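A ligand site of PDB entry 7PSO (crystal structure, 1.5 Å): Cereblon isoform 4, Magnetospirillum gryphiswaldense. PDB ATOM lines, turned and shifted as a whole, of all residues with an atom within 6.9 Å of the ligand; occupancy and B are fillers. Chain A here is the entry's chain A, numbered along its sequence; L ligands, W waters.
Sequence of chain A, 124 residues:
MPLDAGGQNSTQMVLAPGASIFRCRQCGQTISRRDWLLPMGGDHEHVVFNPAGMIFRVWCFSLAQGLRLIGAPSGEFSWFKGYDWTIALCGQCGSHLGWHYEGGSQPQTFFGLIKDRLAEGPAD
The backbone NH of Trp 85 is in hydrogen-bond range of the backbone carbonyl oxygen of Ser 74, 2.8 Å away.
The backbone NH of Met 54 is in hydrogen-bond range of the side-chain amide oxygen of Asn 50, 2.9 Å away.
The backbone carbonyl oxygen of Glu 76 is in hydrogen-bond range of the indole nitrogen of Trp 85 (2.8 Å).
The backbone carbonyl oxygen (O) of Phe 80 is in hydrogen-bond range of the side-chain hydroxyl (OG) of Ser 78 (3.1 Å).
The backbone carbonyl oxygen of Tyr 83 lies within hydrogen-bond range of the side-chain hydroxyl of Ser 78.
N of Glu 76 sits at hydrogen-bond distance from OG of Ser 74.
The indole nitrogen (NE1) of Trp 79 is in hydrogen-bond range of the backbone carbonyl oxygen (O) of Phe 49.
The backbone NH (N) of Ala 52 is in hydrogen-bond range of the side-chain amide oxygen (OD1) of Asn 50 (3.0 Å).
Residues that only touch the ligand: Trp 99 (3.4 Å), Trp 85 (3.4 Å), Ser 78 (3.5 Å), Pro 51 (3.6 Å) and Glu 76 (3.8 Å).
Hydrophobic or aromatic side chains that line the ligand: Pro 51, Phe 77, Trp 79, Trp 85, Trp 99 and Tyr 101.
OH of Tyr 101 is in hydrogen-bond range of O2 of the ligand (2.8 Å).
O of Phe 77 sits at hydrogen-bond distance from N1 of the ligand.
The side-chain amide nitrogen (ND2) of Asn 50 is in hydrogen-bond range of an oxygen (O4) of the ligand (3.1 Å).
N of Trp 79 is in hydrogen-bond range of O2 of the ligand.
Water W1 lies within hydrogen-bond range of the indole nitrogen (NE1) of Trp 99 (3.0 Å) and an oxygen (O4) of the ligand (3.4 Å).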
ATOM      1  N   VAL A  48      19.764 -12.460 -13.218  1.00  0.00           N
ATOM      2  CA  VAL A  48      19.732 -12.266 -11.757  1.00  0.00           C
ATOM      3  C   VAL A  48      18.310 -12.017 -11.301  1.00  0.00           C
ATOM      4  O   VAL A  48      17.486 -11.613 -12.139  1.00  0.00           O
ATOM      5  CB  VAL A  48      20.671 -11.094 -11.389  1.00  0.00           C
ATOM      6  CG1 VAL A  48      22.091 -11.383 -11.781  1.00  0.00           C
ATOM      7  CG2 VAL A  48      20.243  -9.798 -12.098  1.00  0.00           C
ATOM      8  N   PHE A  49      18.037 -12.157 -10.008  1.00  0.00           N
ATOM      9  CA  PHE A  49      16.780 -11.719  -9.382  1.00  0.00           C
ATOM     10  C   PHE A  49      17.016 -10.865  -8.195  1.00  0.00           C
ATOM     11  O   PHE A  49      18.007 -11.104  -7.453  1.00  0.00           O
ATOM     12  CB  PHE A  49      15.996 -12.937  -8.852  1.00  0.00           C
ATOM     13  CG  PHE A  49      15.664 -13.961  -9.884  1.00  0.00           C
ATOM     14  CD1 PHE A  49      16.588 -14.914 -10.285  1.00  0.00           C
ATOM     15  CD2 PHE A  49      14.398 -13.983 -10.429  1.00  0.00           C
ATOM     16  CE1 PHE A  49      16.223 -15.850 -11.240  1.00  0.00           C
ATOM     17  CE2 PHE A  49      14.048 -14.909 -11.404  1.00  0.00           C
ATOM     18  CZ  PHE A  49      14.959 -15.849 -11.790  1.00  0.00           C
ATOM     19  N   ASN A  50      16.130  -9.946  -7.943  1.00  0.00           N
ATOM     20  CA  ASN A  50      16.110  -9.088  -6.752  1.00  0.00           C
ATOM     21  C   ASN A  50      15.282  -9.771  -5.660  1.00  0.00           C
ATOM     22  O   ASN A  50      14.675 -10.816  -5.870  1.00  0.00           O
ATOM     23  CB  ASN A  50      15.723  -7.652  -7.095  1.00  0.00           C
ATOM     24  CG  ASN A  50      14.284  -7.509  -7.532  1.00  0.00           C
ATOM     25  OD1 ASN A  50      13.471  -8.445  -7.391  1.00  0.00           O
ATOM     26  ND2 ASN A  50      13.935  -6.317  -8.007  1.00  0.00           N
ATOM     27  N   PRO A  51      15.228  -9.153  -4.464  1.00  0.00           N
ATOM     28  CA  PRO A  51      14.464  -9.742  -3.362  1.00  0.00           C
ATOM     29  C   PRO A  51      12.975  -9.823  -3.674  1.00  0.00           C
ATOM     30  O   PRO A  51      12.304 -10.625  -3.030  1.00  0.00           O
ATOM     31  CB  PRO A  51      14.764  -8.774  -2.203  1.00  0.00           C
ATOM     32  CG  PRO A  51      16.145  -8.190  -2.540  1.00  0.00           C
ATOM     33  CD  PRO A  51      16.083  -8.026  -4.030  1.00  0.00           C
ATOM     34  N   ALA A  52      12.451  -9.017  -4.600  1.00  0.00           N
ATOM     35  CA  ALA A  52      11.018  -9.037  -4.991  1.00  0.00           C
ATOM     36  C   ALA A  52      10.786 -10.116  -6.062  1.00  0.00           C
ATOM     37  O   ALA A  52       9.693 -10.158  -6.652  1.00  0.00           O
ATOM     38  CB  ALA A  52      10.565  -7.688  -5.445  1.00  0.00           C
ATOM     39  N   MET A  54      11.946 -10.241  -9.115  1.00  0.00           N
ATOM     40  CA  MET A  54      11.977  -9.767 -10.521  1.00  0.00           C
ATOM     41  C   MET A  54      13.266 -10.295 -11.141  1.00  0.00           C
ATOM     42  O   MET A  54      14.375 -10.151 -10.469  1.00  0.00           O
ATOM     43  CB  MET A  54      11.956  -8.248 -10.628  1.00  0.00           C
ATOM     44  CG  MET A  54      10.823  -7.579  -9.869  1.00  0.00           C
ATOM     45  SD  MET A  54      10.784  -5.801 -10.227  1.00  0.00           S
ATOM     46  CE  MET A  54      10.822  -5.132  -8.558  1.00  0.00           C
ATOM     47  N   PHE A  56      16.155 -10.133 -14.075  1.00  0.00           N
ATOM     48  CA  PHE A  56      16.743  -9.142 -15.027  1.00  0.00           C
ATOM     49  C   PHE A  56      17.802  -9.830 -15.839  1.00  0.00           C
ATOM     50  O   PHE A  56      18.669 -10.526 -15.270  1.00  0.00           O
ATOM     51  CB  PHE A  56      17.375  -7.968 -14.315  1.00  0.00           C
ATOM     52  CG  PHE A  56      16.466  -7.222 -13.380  1.00  0.00           C
ATOM     53  CD1 PHE A  56      15.647  -6.204 -13.844  1.00  0.00           C
ATOM     54  CD2 PHE A  56      16.372  -7.565 -12.048  1.00  0.00           C
ATOM     55  CE1 PHE A  56      14.842  -5.497 -12.967  1.00  0.00           C
ATOM     56  CE2 PHE A  56      15.568  -6.865 -11.183  1.00  0.00           C
ATOM     57  CZ  PHE A  56      14.786  -5.827 -11.639  1.00  0.00           C
ATOM     58  N   SER A  74      25.429   0.982  -2.223  1.00  0.00           N
ATOM     59  CA  SER A  74      24.991  -0.040  -1.263  1.00  0.00           C
ATOM     60  C   SER A  74      25.554  -1.395  -1.681  1.00  0.00           C
ATOM     61  O   SER A  74      25.530  -1.725  -2.871  1.00  0.00           O
ATOM     62  CB  SER A  74      23.479  -0.122  -1.166  1.00  0.00           C
ATOM     63  OG  SER A  74      23.122  -1.153  -0.273  1.00  0.00           O
ATOM     64  N   GLY A  75      26.019  -2.211  -0.747  1.00  0.00           N
ATOM     65  CA  GLY A  75      26.448  -3.577  -1.041  1.00  0.00           C
ATOM     66  C   GLY A  75      25.326  -4.583  -0.842  1.00  0.00           C
ATOM     67  O   GLY A  75      25.532  -5.725  -1.223  1.00  0.00           O
ATOM     68  N   GLU A  76      24.180  -4.157  -0.321  1.00  0.00           N
ATOM     69  CA  GLU A  76      23.043  -5.047   0.031  1.00  0.00           C
ATOM     70  C   GLU A  76      22.588  -5.803  -1.211  1.00  0.00           C
ATOM     71  O   GLU A  76      22.256  -5.151  -2.224  1.00  0.00           O
ATOM     72  CB  GLU A  76      21.906  -4.274   0.679  1.00  0.00           C
ATOM     73  CG  GLU A  76      22.298  -3.759   2.054  1.00  0.00           C
ATOM     74  CD  GLU A  76      21.273  -2.939   2.818  1.00  0.00           C
ATOM     75  OE1 GLU A  76      20.197  -2.650   2.268  1.00  0.00           O
ATOM     76  OE2 GLU A  76      21.576  -2.567   3.980  1.00  0.00           O
ATOM     77  N   PHE A  77      22.571  -7.127  -1.148  1.00  0.00           N
ATOM     78  CA  PHE A  77      22.073  -8.046  -2.200  1.00  0.00           C
ATOM     79  C   PHE A  77      22.879  -7.881  -3.487  1.00  0.00           C
ATOM     80  O   PHE A  77      22.385  -8.255  -4.544  1.00  0.00           O
ATOM     81  CB  PHE A  77      20.608  -7.768  -2.530  1.00  0.00           C
ATOM     82  CG  PHE A  77      19.670  -7.890  -1.357  1.00  0.00           C
ATOM     83  CD1 PHE A  77      19.446  -9.112  -0.758  1.00  0.00           C
ATOM     84  CD2 PHE A  77      19.064  -6.776  -0.819  1.00  0.00           C
ATOM     85  CE1 PHE A  77      18.597  -9.212   0.322  1.00  0.00           C
ATOM     86  CE2 PHE A  77      18.217  -6.879   0.270  1.00  0.00           C
ATOM     87  CZ  PHE A  77      17.988  -8.095   0.840  1.00  0.00           C
ATOM     88  N   SER A  78      24.076  -7.306  -3.452  1.00  0.00           N
ATOM     89  CA  SER A  78      24.880  -7.147  -4.677  1.00  0.00           C
ATOM     90  C   SER A  78      25.038  -8.439  -5.437  1.00  0.00           C
ATOM     91  O   SER A  78      25.471  -9.485  -4.881  1.00  0.00           O
ATOM     92  CB  SER A  78      26.223  -6.513  -4.456  1.00  0.00           C
ATOM     93  OG  SER A  78      26.832  -6.325  -5.735  1.00  0.00           O
ATOM     94  N   TRP A  79      24.713  -8.414  -6.725  1.00  0.00           N
ATOM     95  CA  TRP A  79      24.885  -9.546  -7.650  1.00  0.00           C
ATOM     96  C   TRP A  79      26.329  -9.771  -8.011  1.00  0.00           C
ATOM     97  O   TRP A  79      26.638 -10.789  -8.643  1.00  0.00           O
ATOM     98  CB  TRP A  79      24.048  -9.346  -8.905  1.00  0.00           C
ATOM     99  CG  TRP A  79      22.592  -9.322  -8.617  1.00  0.00           C
ATOM    100  CD1 TRP A  79      21.841 -10.206  -7.884  1.00  0.00           C
ATOM    101  CD2 TRP A  79      21.671  -8.367  -9.161  1.00  0.00           C
ATOM    102  NE1 TRP A  79      20.516  -9.853  -7.930  1.00  0.00           N
ATOM    103  CE2 TRP A  79      20.385  -8.733  -8.719  1.00  0.00           C
ATOM    104  CE3 TRP A  79      21.796  -7.269 -10.009  1.00  0.00           C
ATOM    105  CZ2 TRP A  79      19.254  -8.010  -9.060  1.00  0.00           C
ATOM    106  CZ3 TRP A  79      20.680  -6.585 -10.351  1.00  0.00           C
ATOM    107  CH2 TRP A  79      19.418  -6.920  -9.875  1.00  0.00           C
ATOM    108  N   PHE A  80      27.221  -8.822  -7.715  1.00  0.00           N
ATOM    109  CA  PHE A  80      28.613  -8.906  -8.213  1.00  0.00           C
ATOM    110  C   PHE A  80      29.534  -8.742  -7.006  1.00  0.00           C
ATOM    111  O   PHE A  80      29.499  -7.705  -6.323  1.00  0.00           O
ATOM    112  CB  PHE A  80      28.905  -7.858  -9.278  1.00  0.00           C
ATOM    113  CG  PHE A  80      28.078  -8.026 -10.522  1.00  0.00           C
ATOM    114  CD1 PHE A  80      28.543  -8.780 -11.580  1.00  0.00           C
ATOM    115  CD2 PHE A  80      26.902  -7.329 -10.664  1.00  0.00           C
ATOM    116  CE1 PHE A  80      27.810  -8.893 -12.756  1.00  0.00           C
ATOM    117  CE2 PHE A  80      26.135  -7.459 -11.817  1.00  0.00           C
ATOM    118  CZ  PHE A  80      26.602  -8.222 -12.877  1.00  0.00           C
ATOM    119  N   TYR A  83      31.388  -5.499  -5.195  1.00  0.00           N
ATOM    120  CA  TYR A  83      30.834  -4.218  -5.719  1.00  0.00           C
ATOM    121  C   TYR A  83      29.622  -3.781  -4.957  1.00  0.00           C
ATOM    122  O   TYR A  83      28.798  -4.602  -4.539  1.00  0.00           O
ATOM    123  CB  TYR A  83      30.477  -4.334  -7.200  1.00  0.00           C
ATOM    124  CG  TYR A  83      31.604  -4.659  -8.110  1.00  0.00           C
ATOM    125  CD1 TYR A  83      31.954  -5.971  -8.378  1.00  0.00           C
ATOM    126  CD2 TYR A  83      32.400  -3.662  -8.649  1.00  0.00           C
ATOM    127  CE1 TYR A  83      32.990  -6.295  -9.241  1.00  0.00           C
ATOM    128  CE2 TYR A  83      33.441  -3.966  -9.499  1.00  0.00           C
ATOM    129  CZ  TYR A  83      33.765  -5.297  -9.766  1.00  0.00           C
ATOM    130  OH  TYR A  83      34.787  -5.601 -10.601  1.00  0.00           O
ATOM    131  N   TRP A  85      26.426  -0.950  -5.357  1.00  0.00           N
ATOM    132  CA  TRP A  85      25.594  -0.490  -6.525  1.00  0.00           C
ATOM    133  C   TRP A  85      24.866   0.794  -6.198  1.00  0.00           C
ATOM    134  O   TRP A  85      24.537   1.055  -5.045  1.00  0.00           O
ATOM    135  CB  TRP A  85      24.617  -1.576  -6.971  1.00  0.00           C
ATOM    136  CG  TRP A  85      23.709  -2.094  -5.900  1.00  0.00           C
ATOM    137  CD1 TRP A  85      23.931  -3.220  -5.181  1.00  0.00           C
ATOM    138  CD2 TRP A  85      22.523  -1.489  -5.365  1.00  0.00           C
ATOM    139  NE1 TRP A  85      22.949  -3.376  -4.246  1.00  0.00           N
ATOM    140  CE2 TRP A  85      22.073  -2.324  -4.309  1.00  0.00           C
ATOM    141  CE3 TRP A  85      21.747  -0.356  -5.645  1.00  0.00           C
ATOM    142  CZ2 TRP A  85      20.940  -2.062  -3.567  1.00  0.00           C
ATOM    143  CZ3 TRP A  85      20.615  -0.101  -4.916  1.00  0.00           C
ATOM    144  CH2 TRP A  85      20.200  -0.957  -3.901  1.00  0.00           C
ATOM    145  N   THR A  86      24.563   1.529  -7.281  1.00  0.00           N
ATOM    146  CA  THR A  86      23.636   2.681  -7.292  1.00  0.00           C
ATOM    147  C   THR A  86      22.684   2.439  -8.449  1.00  0.00           C
ATOM    148  O   THR A  86      23.104   1.925  -9.445  1.00  0.00           O
ATOM    149  CB  THR A  86      24.290   4.045  -7.435  1.00  0.00           C
ATOM    150  OG1 THR A  86      25.082   4.093  -8.631  1.00  0.00           O
ATOM    151  CG2 THR A  86      25.085   4.373  -6.180  1.00  0.00           C
ATOM    152  N   ILE A  87      21.438   2.731  -8.221  1.00  0.00           N
ATOM    153  CA  ILE A  87      20.419   2.705  -9.298  1.00  0.00           C
ATOM    154  C   ILE A  87      20.842   3.673 -10.392  1.00  0.00           C
ATOM    155  O   ILE A  87      21.218   4.832 -10.076  1.00  0.00           O
ATOM    156  CB  ILE A  87      19.059   3.032  -8.700  1.00  0.00           C
ATOM    157  CG1 ILE A  87      18.573   1.872  -7.845  1.00  0.00           C
ATOM    158  CG2 ILE A  87      18.066   3.359  -9.806  1.00  0.00           C
ATOM    159  CD1 ILE A  87      17.391   2.261  -6.953  1.00  0.00           C
ATOM    160  N   HIS A  96      14.138   3.134 -15.338  1.00  0.00           N
ATOM    161  CA  HIS A  96      15.196   2.383 -14.628  1.00  0.00           C
ATOM    162  C   HIS A  96      15.947   1.474 -15.582  1.00  0.00           C
ATOM    163  O   HIS A  96      15.422   0.461 -16.048  1.00  0.00           O
ATOM    164  CB  HIS A  96      14.591   1.625 -13.476  1.00  0.00           C
ATOM    165  CG  HIS A  96      15.621   0.821 -12.803  1.00  0.00           C
ATOM    166  ND1 HIS A  96      15.297  -0.334 -12.131  1.00  0.00           N
ATOM    167  CD2 HIS A  96      16.953   1.043 -12.631  1.00  0.00           C
ATOM    168  CE1 HIS A  96      16.405  -0.810 -11.576  1.00  0.00           C
ATOM    169  NE2 HIS A  96      17.428  -0.010 -11.886  1.00  0.00           N
ATOM    170  N   TRP A  99      22.057  -0.414 -13.096  1.00  0.00           N
ATOM    171  CA  TRP A  99      22.866  -0.054 -11.899  1.00  0.00           C
ATOM    172  C   TRP A  99      24.287   0.296 -12.326  1.00  0.00           C
ATOM    173  O   TRP A  99      24.798  -0.262 -13.296  1.00  0.00           O
ATOM    174  CB  TRP A  99      22.864  -1.215 -10.878  1.00  0.00           C
ATOM    175  CG  TRP A  99      21.492  -1.667 -10.420  1.00  0.00           C
ATOM    176  CD1 TRP A  99      20.797  -1.176  -9.381  1.00  0.00           C
ATOM    177  CD2 TRP A  99      20.603  -2.550 -11.106  1.00  0.00           C
ATOM    178  NE1 TRP A  99      19.561  -1.760  -9.308  1.00  0.00           N
ATOM    179  CE2 TRP A  99      19.426  -2.615 -10.336  1.00  0.00           C
ATOM    180  CE3 TRP A  99      20.724  -3.373 -12.233  1.00  0.00           C
ATOM    181  CZ2 TRP A  99      18.343  -3.431 -10.704  1.00  0.00           C
ATOM    182  CZ3 TRP A  99      19.632  -4.114 -12.645  1.00  0.00           C
ATOM    183  CH2 TRP A  99      18.488  -4.149 -11.864  1.00  0.00           C
ATOM    184  N   TYR A 101      28.027  -0.026 -10.684  1.00  0.00           N
ATOM    185  CA  TYR A 101      28.795  -0.808  -9.681  1.00  0.00           C
ATOM    186  C   TYR A 101      30.149  -0.109  -9.448  1.00  0.00           C
ATOM    187  O   TYR A 101      30.751   0.339 -10.419  1.00  0.00           O
ATOM    188  CB  TYR A 101      28.938  -2.237 -10.199  1.00  0.00           C
ATOM    189  CG  TYR A 101      27.623  -2.997 -10.130  1.00  0.00           C
ATOM    190  CD1 TYR A 101      27.189  -3.561  -8.934  1.00  0.00           C
ATOM    191  CD2 TYR A 101      26.804  -3.020 -11.219  1.00  0.00           C
ATOM    192  CE1 TYR A 101      25.987  -4.250  -8.879  1.00  0.00           C
ATOM    193  CE2 TYR A 101      25.600  -3.706 -11.174  1.00  0.00           C
ATOM    194  CZ  TYR A 101      25.176  -4.306  -9.998  1.00  0.00           C
ATOM    195  OH  TYR A 101      23.967  -4.959  -9.882  1.00  0.00           O
HETATM  196  O1  LIG L   1      19.041  -7.190  -5.830  1.00  0.00           O
HETATM  197  C1  LIG L   1      19.775  -6.312  -6.323  1.00  0.00           C
HETATM  198  N1  LIG L   1      21.093  -6.483  -6.473  1.00  0.00           N
HETATM  199  C2  LIG L   1      21.940  -5.631  -7.096  1.00  0.00           C
HETATM  200  O2  LIG L   1      23.055  -5.895  -7.377  1.00  0.00           O
HETATM  201  C3  LIG L   1      21.332  -4.340  -7.598  1.00  0.00           C
HETATM  202  C4  LIG L   1      20.145  -3.898  -6.787  1.00  0.00           C
HETATM  203  C5  LIG L   1      19.134  -5.071  -6.799  1.00  0.00           C
HETATM  204  N2  LIG L   1      17.962  -4.709  -5.998  1.00  0.00           N
HETATM  205  C6  LIG L   1      14.521  -3.650  -3.010  1.00  0.00           C
HETATM  206  C7  LIG L   1      15.876  -3.974  -2.993  1.00  0.00           C
HETATM  207  C8  LIG L   1      16.452  -4.234  -4.220  1.00  0.00           C
HETATM  208  C9  LIG L   1      15.710  -4.124  -5.470  1.00  0.00           C
HETATM  209  O3  LIG L   1      18.831  -4.765  -3.896  1.00  0.00           O
HETATM  210  O4  LIG L   1      16.495  -4.559  -7.789  1.00  0.00           O
HETATM  211  C10 LIG L   1      14.377  -3.823  -5.454  1.00  0.00           C
HETATM  212  C11 LIG L   1      13.787  -3.581  -4.218  1.00  0.00           C
HETATM  213  C12 LIG L   1      16.710  -4.448  -6.493  1.00  0.00           C
HETATM  214  C13 LIG L   1      17.806  -4.599  -4.690  1.00  0.00           C
HETATM  215  O   HOH W   1      17.461  -1.317  -7.269  1.00  0.00           O
HETATM  216  O   HOH W   2      18.692  -3.132  -1.402  1.00  0.00           O
